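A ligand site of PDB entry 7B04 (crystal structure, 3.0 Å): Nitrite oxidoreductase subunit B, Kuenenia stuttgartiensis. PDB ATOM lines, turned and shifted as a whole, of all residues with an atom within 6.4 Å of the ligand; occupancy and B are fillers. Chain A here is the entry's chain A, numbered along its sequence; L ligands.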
ATOM      1  N   PHE A  26      18.767  25.344  -3.827  1.00  0.00           N
ATOM      2  CA  PHE A  26      18.173  24.471  -2.810  1.00  0.00           C
ATOM      3  C   PHE A  26      18.145  23.044  -3.326  1.00  0.00           C
ATOM      4  O   PHE A  26      17.511  22.755  -4.347  1.00  0.00           O
ATOM      5  CB  PHE A  26      16.763  24.963  -2.467  1.00  0.00           C
ATOM      6  CG  PHE A  26      15.986  24.022  -1.575  1.00  0.00           C
ATOM      7  CD1 PHE A  26      15.179  23.036  -2.111  1.00  0.00           C
ATOM      8  CD2 PHE A  26      16.069  24.138  -0.203  1.00  0.00           C
ATOM      9  CE1 PHE A  26      14.468  22.176  -1.294  1.00  0.00           C
ATOM     10  CE2 PHE A  26      15.354  23.286   0.611  1.00  0.00           C
ATOM     11  CZ  PHE A  26      14.556  22.305   0.078  1.00  0.00           C
ATOM     12  N   CYS A  41       7.645  12.368   6.778  1.00  0.00           N
ATOM     13  CA  CYS A  41       7.803  13.579   5.992  1.00  0.00           C
ATOM     14  C   CYS A  41       6.474  14.030   5.401  1.00  0.00           C
ATOM     15  O   CYS A  41       6.201  15.238   5.311  1.00  0.00           O
ATOM     16  CB  CYS A  41       8.818  13.352   4.878  1.00  0.00           C
ATOM     17  SG  CYS A  41       8.585  11.797   3.982  1.00  0.00           S
ATOM     18  N   ALA A  44       4.566  15.791   7.965  1.00  0.00           N
ATOM     19  CA  ALA A  44       5.237  17.036   8.303  1.00  0.00           C
ATOM     20  C   ALA A  44       4.714  18.189   7.466  1.00  0.00           C
ATOM     21  O   ALA A  44       4.355  19.249   7.999  1.00  0.00           O
ATOM     22  CB  ALA A  44       6.751  16.880   8.123  1.00  0.00           C
ATOM     23  N   CYS A  45       4.652  18.000   6.151  1.00  0.00           N
ATOM     24  CA  CYS A  45       4.154  19.046   5.278  1.00  0.00           C
ATOM     25  C   CYS A  45       2.649  19.235   5.445  1.00  0.00           C
ATOM     26  O   CYS A  45       2.148  20.367   5.411  1.00  0.00           O
ATOM     27  CB  CYS A  45       4.492  18.722   3.822  1.00  0.00           C
ATOM     28  SG  CYS A  45       3.974  19.976   2.635  1.00  0.00           S
ATOM     29  N   LYS A  46       1.914  18.133   5.618  1.00  0.00           N
ATOM     30  CA  LYS A  46       0.458  18.222   5.737  1.00  0.00           C
ATOM     31  C   LYS A  46       0.047  19.043   6.946  1.00  0.00           C
ATOM     32  O   LYS A  46      -0.726  20.004   6.833  1.00  0.00           O
ATOM     33  CB  LYS A  46      -0.139  16.813   5.796  1.00  0.00           C
ATOM     34  CG  LYS A  46      -1.604  16.780   6.244  1.00  0.00           C
ATOM     35  CD  LYS A  46      -2.502  17.543   5.288  1.00  0.00           C
ATOM     36  CE  LYS A  46      -2.688  16.806   3.973  1.00  0.00           C
ATOM     37  NZ  LYS A  46      -3.659  17.476   3.069  1.00  0.00           N
ATOM     38  N   THR A  48       1.361  21.302   8.387  1.00  0.00           N
ATOM     39  CA  THR A  48       1.951  22.633   8.406  1.00  0.00           C
ATOM     40  C   THR A  48       1.411  23.560   7.326  1.00  0.00           C
ATOM     41  O   THR A  48       1.180  24.733   7.584  1.00  0.00           O
ATOM     42  CB  THR A  48       3.483  22.531   8.258  1.00  0.00           C
ATOM     43  OG1 THR A  48       3.986  21.606   9.232  1.00  0.00           O
ATOM     44  CG2 THR A  48       4.138  23.882   8.469  1.00  0.00           C
ATOM     45  N   TRP A  49       1.185  23.049   6.107  1.00  0.00           N
ATOM     46  CA  TRP A  49       0.843  23.906   4.983  1.00  0.00           C
ATOM     47  C   TRP A  49      -0.453  23.535   4.280  1.00  0.00           C
ATOM     48  O   TRP A  49      -1.147  24.435   3.791  1.00  0.00           O
ATOM     49  CB  TRP A  49       1.964  23.877   3.936  1.00  0.00           C
ATOM     50  CG  TRP A  49       3.325  24.214   4.474  1.00  0.00           C
ATOM     51  CD1 TRP A  49       4.393  23.368   4.588  1.00  0.00           C
ATOM     52  CD2 TRP A  49       3.767  25.482   4.950  1.00  0.00           C
ATOM     53  NE1 TRP A  49       5.465  24.037   5.112  1.00  0.00           N
ATOM     54  CE2 TRP A  49       5.113  25.334   5.348  1.00  0.00           C
ATOM     55  CE3 TRP A  49       3.148  26.734   5.097  1.00  0.00           C
ATOM     56  CZ2 TRP A  49       5.849  26.389   5.874  1.00  0.00           C
ATOM     57  CZ3 TRP A  49       3.892  27.779   5.616  1.00  0.00           C
ATOM     58  CH2 TRP A  49       5.224  27.598   6.003  1.00  0.00           C
ATOM     59  N   THR A  50      -0.816  22.251   4.221  1.00  0.00           N
ATOM     60  CA  THR A  50      -1.956  21.800   3.436  1.00  0.00           C
ATOM     61  C   THR A  50      -3.015  21.137   4.317  1.00  0.00           C
ATOM     62  O   THR A  50      -3.634  20.150   3.931  1.00  0.00           O
ATOM     63  CB  THR A  50      -1.518  20.845   2.330  1.00  0.00           C
ATOM     64  OG1 THR A  50      -1.431  19.512   2.849  1.00  0.00           O
ATOM     65  CG2 THR A  50      -0.156  21.255   1.777  1.00  0.00           C
ATOM     66  N   TRP A  60       1.828  17.634  -0.798  1.00  0.00           N
ATOM     67  CA  TRP A  60       3.023  18.150  -1.491  1.00  0.00           C
ATOM     68  C   TRP A  60       4.155  17.142  -1.297  1.00  0.00           C
ATOM     69  O   TRP A  60       4.828  16.859  -2.232  1.00  0.00           O
ATOM     70  CB  TRP A  60       3.373  19.548  -0.991  1.00  0.00           C
ATOM     71  CG  TRP A  60       2.300  20.573  -1.207  1.00  0.00           C
ATOM     72  CD1 TRP A  60       1.228  20.472  -2.026  1.00  0.00           C
ATOM     73  CD2 TRP A  60       2.208  21.865  -0.608  1.00  0.00           C
ATOM     74  NE1 TRP A  60       0.485  21.599  -1.978  1.00  0.00           N
ATOM     75  CE2 TRP A  60       1.053  22.460  -1.104  1.00  0.00           C
ATOM     76  CE3 TRP A  60       2.982  22.566   0.311  1.00  0.00           C
ATOM     77  CZ2 TRP A  60       0.663  23.737  -0.725  1.00  0.00           C
ATOM     78  CZ3 TRP A  60       2.591  23.821   0.693  1.00  0.00           C
ATOM     79  CH2 TRP A  60       1.443  24.391   0.183  1.00  0.00           C
ATOM     80  N   ASN A  61       4.293  16.604  -0.101  1.00  0.00           N
ATOM     81  CA  ASN A  61       5.303  15.541   0.082  1.00  0.00           C
ATOM     82  C   ASN A  61       4.539  14.227   0.125  1.00  0.00           C
ATOM     83  O   ASN A  61       3.557  14.154   0.832  1.00  0.00           O
ATOM     84  CB  ASN A  61       6.149  15.717   1.330  1.00  0.00           C
ATOM     85  CG  ASN A  61       7.136  14.595   1.536  1.00  0.00           C
ATOM     86  OD1 ASN A  61       8.307  14.719   1.205  1.00  0.00           O
ATOM     87  ND2 ASN A  61       6.697  13.482   2.078  1.00  0.00           N
ATOM     88  N   ARG A 173       9.076  12.187  -2.840  1.00  0.00           N
ATOM     89  CA  ARG A 173       8.980  13.263  -3.816  1.00  0.00           C
ATOM     90  C   ARG A 173       8.367  14.518  -3.211  1.00  0.00           C
ATOM     91  O   ARG A 173       7.309  14.454  -2.574  1.00  0.00           O
ATOM     92  CB  ARG A 173       8.149  12.849  -5.036  1.00  0.00           C
ATOM     93  CG  ARG A 173       8.383  11.443  -5.549  1.00  0.00           C
ATOM     94  CD  ARG A 173       7.854  11.316  -6.964  1.00  0.00           C
ATOM     95  NE  ARG A 173       6.407  11.502  -7.026  1.00  0.00           N
ATOM     96  CZ  ARG A 173       5.816  12.615  -7.463  1.00  0.00           C
ATOM     97  NH1 ARG A 173       6.545  13.630  -7.890  1.00  0.00           N
ATOM     98  NH2 ARG A 173       4.488  12.693  -7.485  1.00  0.00           N
ATOM     99  N   ILE A 174       9.027  15.645  -3.445  1.00  0.00           N
ATOM    100  CA  ILE A 174       8.509  16.993  -3.193  1.00  0.00           C
ATOM    101  C   ILE A 174       8.658  17.750  -4.500  1.00  0.00           C
ATOM    102  O   ILE A 174       9.058  17.192  -5.517  1.00  0.00           O
ATOM    103  CB  ILE A 174       9.264  17.736  -2.079  1.00  0.00           C
ATOM    104  CG1 ILE A 174      10.728  17.952  -2.439  1.00  0.00           C
ATOM    105  CG2 ILE A 174       9.236  17.026  -0.816  1.00  0.00           C
ATOM    106  CD1 ILE A 174      11.414  18.895  -1.483  1.00  0.00           C
ATOM    107  N   CYS A 175       8.330  19.040  -4.462  1.00  0.00           N
ATOM    108  CA  CYS A 175       8.695  19.892  -5.579  1.00  0.00           C
ATOM    109  C   CYS A 175      10.206  19.888  -5.721  1.00  0.00           C
ATOM    110  O   CYS A 175      10.940  20.192  -4.770  1.00  0.00           O
ATOM    111  CB  CYS A 175       8.188  21.317  -5.347  1.00  0.00           C
ATOM    112  SG  CYS A 175       8.749  22.456  -6.628  1.00  0.00           S
ATOM    113  N   HIS A 177      11.960  21.900  -7.295  1.00  0.00           N
ATOM    114  CA  HIS A 177      12.441  23.279  -7.422  1.00  0.00           C
ATOM    115  C   HIS A 177      13.441  23.378  -8.570  1.00  0.00           C
ATOM    116  O   HIS A 177      14.604  23.751  -8.416  1.00  0.00           O
ATOM    117  CB  HIS A 177      13.026  23.773  -6.106  1.00  0.00           C
ATOM    118  CG  HIS A 177      11.992  23.952  -5.035  1.00  0.00           C
ATOM    119  ND1 HIS A 177      11.171  25.062  -4.975  1.00  0.00           N
ATOM    120  CD2 HIS A 177      11.626  23.158  -4.008  1.00  0.00           C
ATOM    121  CE1 HIS A 177      10.355  24.948  -3.954  1.00  0.00           C
ATOM    122  NE2 HIS A 177      10.605  23.801  -3.341  1.00  0.00           N
ATOM    123  N   LYS A 234       1.670  25.156  -4.337  1.00  0.00           N
ATOM    124  CA  LYS A 234       2.734  24.183  -4.524  1.00  0.00           C
ATOM    125  C   LYS A 234       3.651  24.207  -3.305  1.00  0.00           C
ATOM    126  O   LYS A 234       3.524  25.069  -2.431  1.00  0.00           O
ATOM    127  CB  LYS A 234       3.542  24.487  -5.796  1.00  0.00           C
ATOM    128  CG  LYS A 234       4.398  25.736  -5.686  1.00  0.00           C
ATOM    129  CD  LYS A 234       5.179  25.982  -6.959  1.00  0.00           C
ATOM    130  CE  LYS A 234       6.324  24.990  -7.107  1.00  0.00           C
ATOM    131  NZ  LYS A 234       7.359  25.185  -6.055  1.00  0.00           N
ATOM    132  N   CYS A 235       4.559  23.241  -3.263  1.00  0.00           N
ATOM    133  CA  CYS A 235       5.573  23.205  -2.223  1.00  0.00           C
ATOM    134  C   CYS A 235       6.397  24.483  -2.244  1.00  0.00           C
ATOM    135  O   CYS A 235       6.927  24.883  -3.281  1.00  0.00           O
ATOM    136  CB  CYS A 235       6.471  21.982  -2.394  1.00  0.00           C
ATOM    137  SG  CYS A 235       8.105  22.126  -1.642  1.00  0.00           S
ATOM    138  N   ILE A 236       6.490  25.136  -1.078  1.00  0.00           N
ATOM    139  CA  ILE A 236       7.211  26.394  -0.942  1.00  0.00           C
ATOM    140  C   ILE A 236       8.623  26.183  -0.391  1.00  0.00           C
ATOM    141  O   ILE A 236       9.304  27.168  -0.078  1.00  0.00           O
ATOM    142  CB  ILE A 236       6.431  27.364  -0.048  1.00  0.00           C
ATOM    143  CG1 ILE A 236       6.356  26.810   1.377  1.00  0.00           C
ATOM    144  CG2 ILE A 236       5.032  27.579  -0.605  1.00  0.00           C
ATOM    145  CD1 ILE A 236       5.886  27.788   2.397  1.00  0.00           C
ATOM    146  N   ALA A 237       9.070  24.938  -0.260  1.00  0.00           N
ATOM    147  CA  ALA A 237      10.354  24.585   0.337  1.00  0.00           C
ATOM    148  C   ALA A 237      10.499  25.137   1.757  1.00  0.00           C
ATOM    149  O   ALA A 237      11.620  25.294   2.243  1.00  0.00           O
ATOM    150  CB  ALA A 237      11.527  25.052  -0.522  1.00  0.00           C
ATOM    151  N   CYS A 238       9.368  25.406   2.411  1.00  0.00           N
ATOM    152  CA  CYS A 238       9.325  26.028   3.744  1.00  0.00           C
ATOM    153  C   CYS A 238      10.335  27.163   3.833  1.00  0.00           C
ATOM    154  O   CYS A 238      11.217  27.189   4.702  1.00  0.00           O
ATOM    155  CB  CYS A 238       9.566  25.003   4.842  1.00  0.00           C
ATOM    156  SG  CYS A 238       8.486  23.556   4.769  1.00  0.00           S
ATOM    157  N   TYR A 239      10.201  28.119   2.918  1.00  0.00           N
ATOM    158  CA  TYR A 239      11.200  29.177   2.816  1.00  0.00           C
ATOM    159  C   TYR A 239      11.346  30.017   4.083  1.00  0.00           C
ATOM    160  O   TYR A 239      12.449  30.539   4.304  1.00  0.00           O
ATOM    161  CB  TYR A 239      10.937  30.049   1.581  1.00  0.00           C
ATOM    162  CG  TYR A 239       9.628  30.810   1.575  1.00  0.00           C
ATOM    163  CD1 TYR A 239       8.461  30.228   1.114  1.00  0.00           C
ATOM    164  CD2 TYR A 239       9.578  32.134   1.997  1.00  0.00           C
ATOM    165  CE1 TYR A 239       7.264  30.927   1.091  1.00  0.00           C
ATOM    166  CE2 TYR A 239       8.394  32.844   1.990  1.00  0.00           C
ATOM    167  CZ  TYR A 239       7.242  32.234   1.530  1.00  0.00           C
ATOM    168  OH  TYR A 239       6.057  32.929   1.514  1.00  0.00           O
ATOM    169  N   THR A 256      14.254  22.263   5.653  1.00  0.00           N
ATOM    170  CA  THR A 256      12.812  22.362   5.509  1.00  0.00           C
ATOM    171  C   THR A 256      12.125  21.315   6.384  1.00  0.00           C
ATOM    172  O   THR A 256      12.709  20.324   6.818  1.00  0.00           O
ATOM    173  CB  THR A 256      12.365  22.243   4.052  1.00  0.00           C
ATOM    174  OG1 THR A 256      10.963  22.517   3.961  1.00  0.00           O
ATOM    175  CG2 THR A 256      12.594  20.898   3.525  1.00  0.00           C
ATOM    176  N   ARG A 257      10.844  21.579   6.616  1.00  0.00           N
ATOM    177  CA  ARG A 257      10.083  20.815   7.593  1.00  0.00           C
ATOM    178  C   ARG A 257       9.975  19.330   7.229  1.00  0.00           C
ATOM    179  O   ARG A 257       9.995  18.472   8.108  1.00  0.00           O
ATOM    180  CB  ARG A 257       8.694  21.435   7.733  1.00  0.00           C
ATOM    181  CG  ARG A 257       7.956  20.832   8.835  1.00  0.00           C
ATOM    182  CD  ARG A 257       7.126  21.764   9.624  1.00  0.00           C
ATOM    183  NE  ARG A 257       6.196  20.948  10.380  1.00  0.00           N
ATOM    184  CZ  ARG A 257       6.574  20.172  11.405  1.00  0.00           C
ATOM    185  NH1 ARG A 257       5.680  19.422  12.020  1.00  0.00           N
ATOM    186  NH2 ARG A 257       7.840  20.173  11.829  1.00  0.00           N
ATOM    187  N   CYS A 258       9.851  19.021   5.941  1.00  0.00           N
ATOM    188  CA  CYS A 258       9.786  17.610   5.539  1.00  0.00           C
ATOM    189  C   CYS A 258      11.139  16.927   5.672  1.00  0.00           C
ATOM    190  O   CYS A 258      11.191  15.719   5.952  1.00  0.00           O
ATOM    191  CB  CYS A 258       9.246  17.494   4.106  1.00  0.00           C
ATOM    192  SG  CYS A 258      10.316  18.202   2.844  1.00  0.00           S
ATOM    193  N   MET A 259      12.240  17.655   5.465  1.00  0.00           N
ATOM    194  CA  MET A 259      13.555  17.039   5.603  1.00  0.00           C
ATOM    195  C   MET A 259      13.882  16.750   7.060  1.00  0.00           C
ATOM    196  O   MET A 259      14.426  15.687   7.378  1.00  0.00           O
ATOM    197  CB  MET A 259      14.647  17.930   4.984  1.00  0.00           C
ATOM    198  CG  MET A 259      14.455  18.254   3.526  1.00  0.00           C
ATOM    199  SD  MET A 259      14.481  16.915   2.329  1.00  0.00           S
ATOM    200  CE  MET A 259      13.982  17.795   0.864  1.00  0.00           C
ATOM    201  N   ARG A 267      17.537  11.605   4.226  1.00  0.00           N
ATOM    202  CA  ARG A 267      17.574  12.859   3.478  1.00  0.00           C
ATOM    203  C   ARG A 267      18.427  13.886   4.194  1.00  0.00           C
ATOM    204  O   ARG A 267      18.300  14.070   5.404  1.00  0.00           O
ATOM    205  CB  ARG A 267      16.170  13.397   3.203  1.00  0.00           C
ATOM    206  CG  ARG A 267      15.309  13.491   4.400  1.00  0.00           C
ATOM    207  CD  ARG A 267      13.935  14.055   4.068  1.00  0.00           C
ATOM    208  NE  ARG A 267      13.202  13.329   3.038  1.00  0.00           N
ATOM    209  CZ  ARG A 267      11.957  13.638   2.678  1.00  0.00           C
ATOM    210  NH1 ARG A 267      11.350  12.937   1.723  1.00  0.00           N
ATOM    211  NH2 ARG A 267      11.326  14.637   3.266  1.00  0.00           N
HETATM  212 FE1  LIG L   1       6.109  20.732   2.610  1.00  0.00          FE
HETATM  213 FE2  LIG L   1       7.651  21.348   0.443  1.00  0.00          FE
HETATM  214 FE3  LIG L   1       8.558  19.559   2.304  1.00  0.00          FE
HETATM  215 FE4  LIG L   1       8.383  22.221   2.934  1.00  0.00          FE
HETATM  216  S1  LIG L   1       9.738  21.265   1.363  1.00  0.00           S
HETATM  217  S2  LIG L   1       7.712  20.462   4.225  1.00  0.00           S
HETATM  218  S3  LIG L   1       6.519  22.812   1.765  1.00  0.00           S
HETATM  219  S4  LIG L   1       6.750  19.309   0.948  1.00  0.00           S
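The side-chain sulfur (SG) of Cys 45 is bound to an iron atom (FE1) of the ligand, at 2.3 Å.
An iron atom (FE4) of the ligand is bound by the side-chain sulfur (SG) of Cys 238, 2.3 Å away.
An iron atom (FE2) of the ligand is bound by the side-chain sulfur (SG) of Cys 235.
N of Cys 258 lies close to S2 of the ligand (3.1 Å).
SG of Cys 258 binds FE3 of the ligand, at 2.3 Å.
The side-chain hydroxyl (OG1) of Thr 256 sits close to a sulfur (S1) of the ligand.
A sulfur (S3) of the ligand lies close to the indole nitrogen (NE1) of Trp 49 (3.7 Å).
The backbone NH (N) of Ile 236 lies close to a sulfur (S3) of the ligand (3.7 Å).
SG of Cys 238 lies close to OG1 of Thr 256 (2.8 Å).
The side-chain sulfur (SG) of Cys 238 lies close to the indole nitrogen (NE1) of Trp 49, 3.1 Å away.
The backbone NH of Arg 257 sits close to the side-chain sulfur of Cys 238 (3.6 Å).
SG of Cys 235 sits close to NE2 of His 177.
The guanidinium group of Arg 267 is in hydrogen-bond range of the backbone carbonyl oxygen of Cys 258.
The backbone carbonyl oxygen (O) of Ala 237 lies within hydrogen-bond range of the side-chain hydroxyl (OG1) of Thr 256 (3.3 Å).
ND2 of Asn 61 lies close to SG of Cys 41 (3.2 Å).
OG1 of Thr 48 sits at hydrogen-bond distance from NE of Arg 257 (2.6 Å).
Trp 60 touches the ligand (CE3 to S3, 3.8 Å).
Asn 61 touches the ligand (CB to S4, 3.7 Å).
Ile 174 touches the ligand (CG2 to S4, 3.8 Å).
Ala 237 touches the ligand.
Arg 257 touches the ligand (CB to S2, 3.8 Å).
Hydrophobic or aromatic side chains that line the ligand: Trp 49, Trp 60 and Ile 174.
Of the 25 residues printed, 12 come within 4 Å of the ligand.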
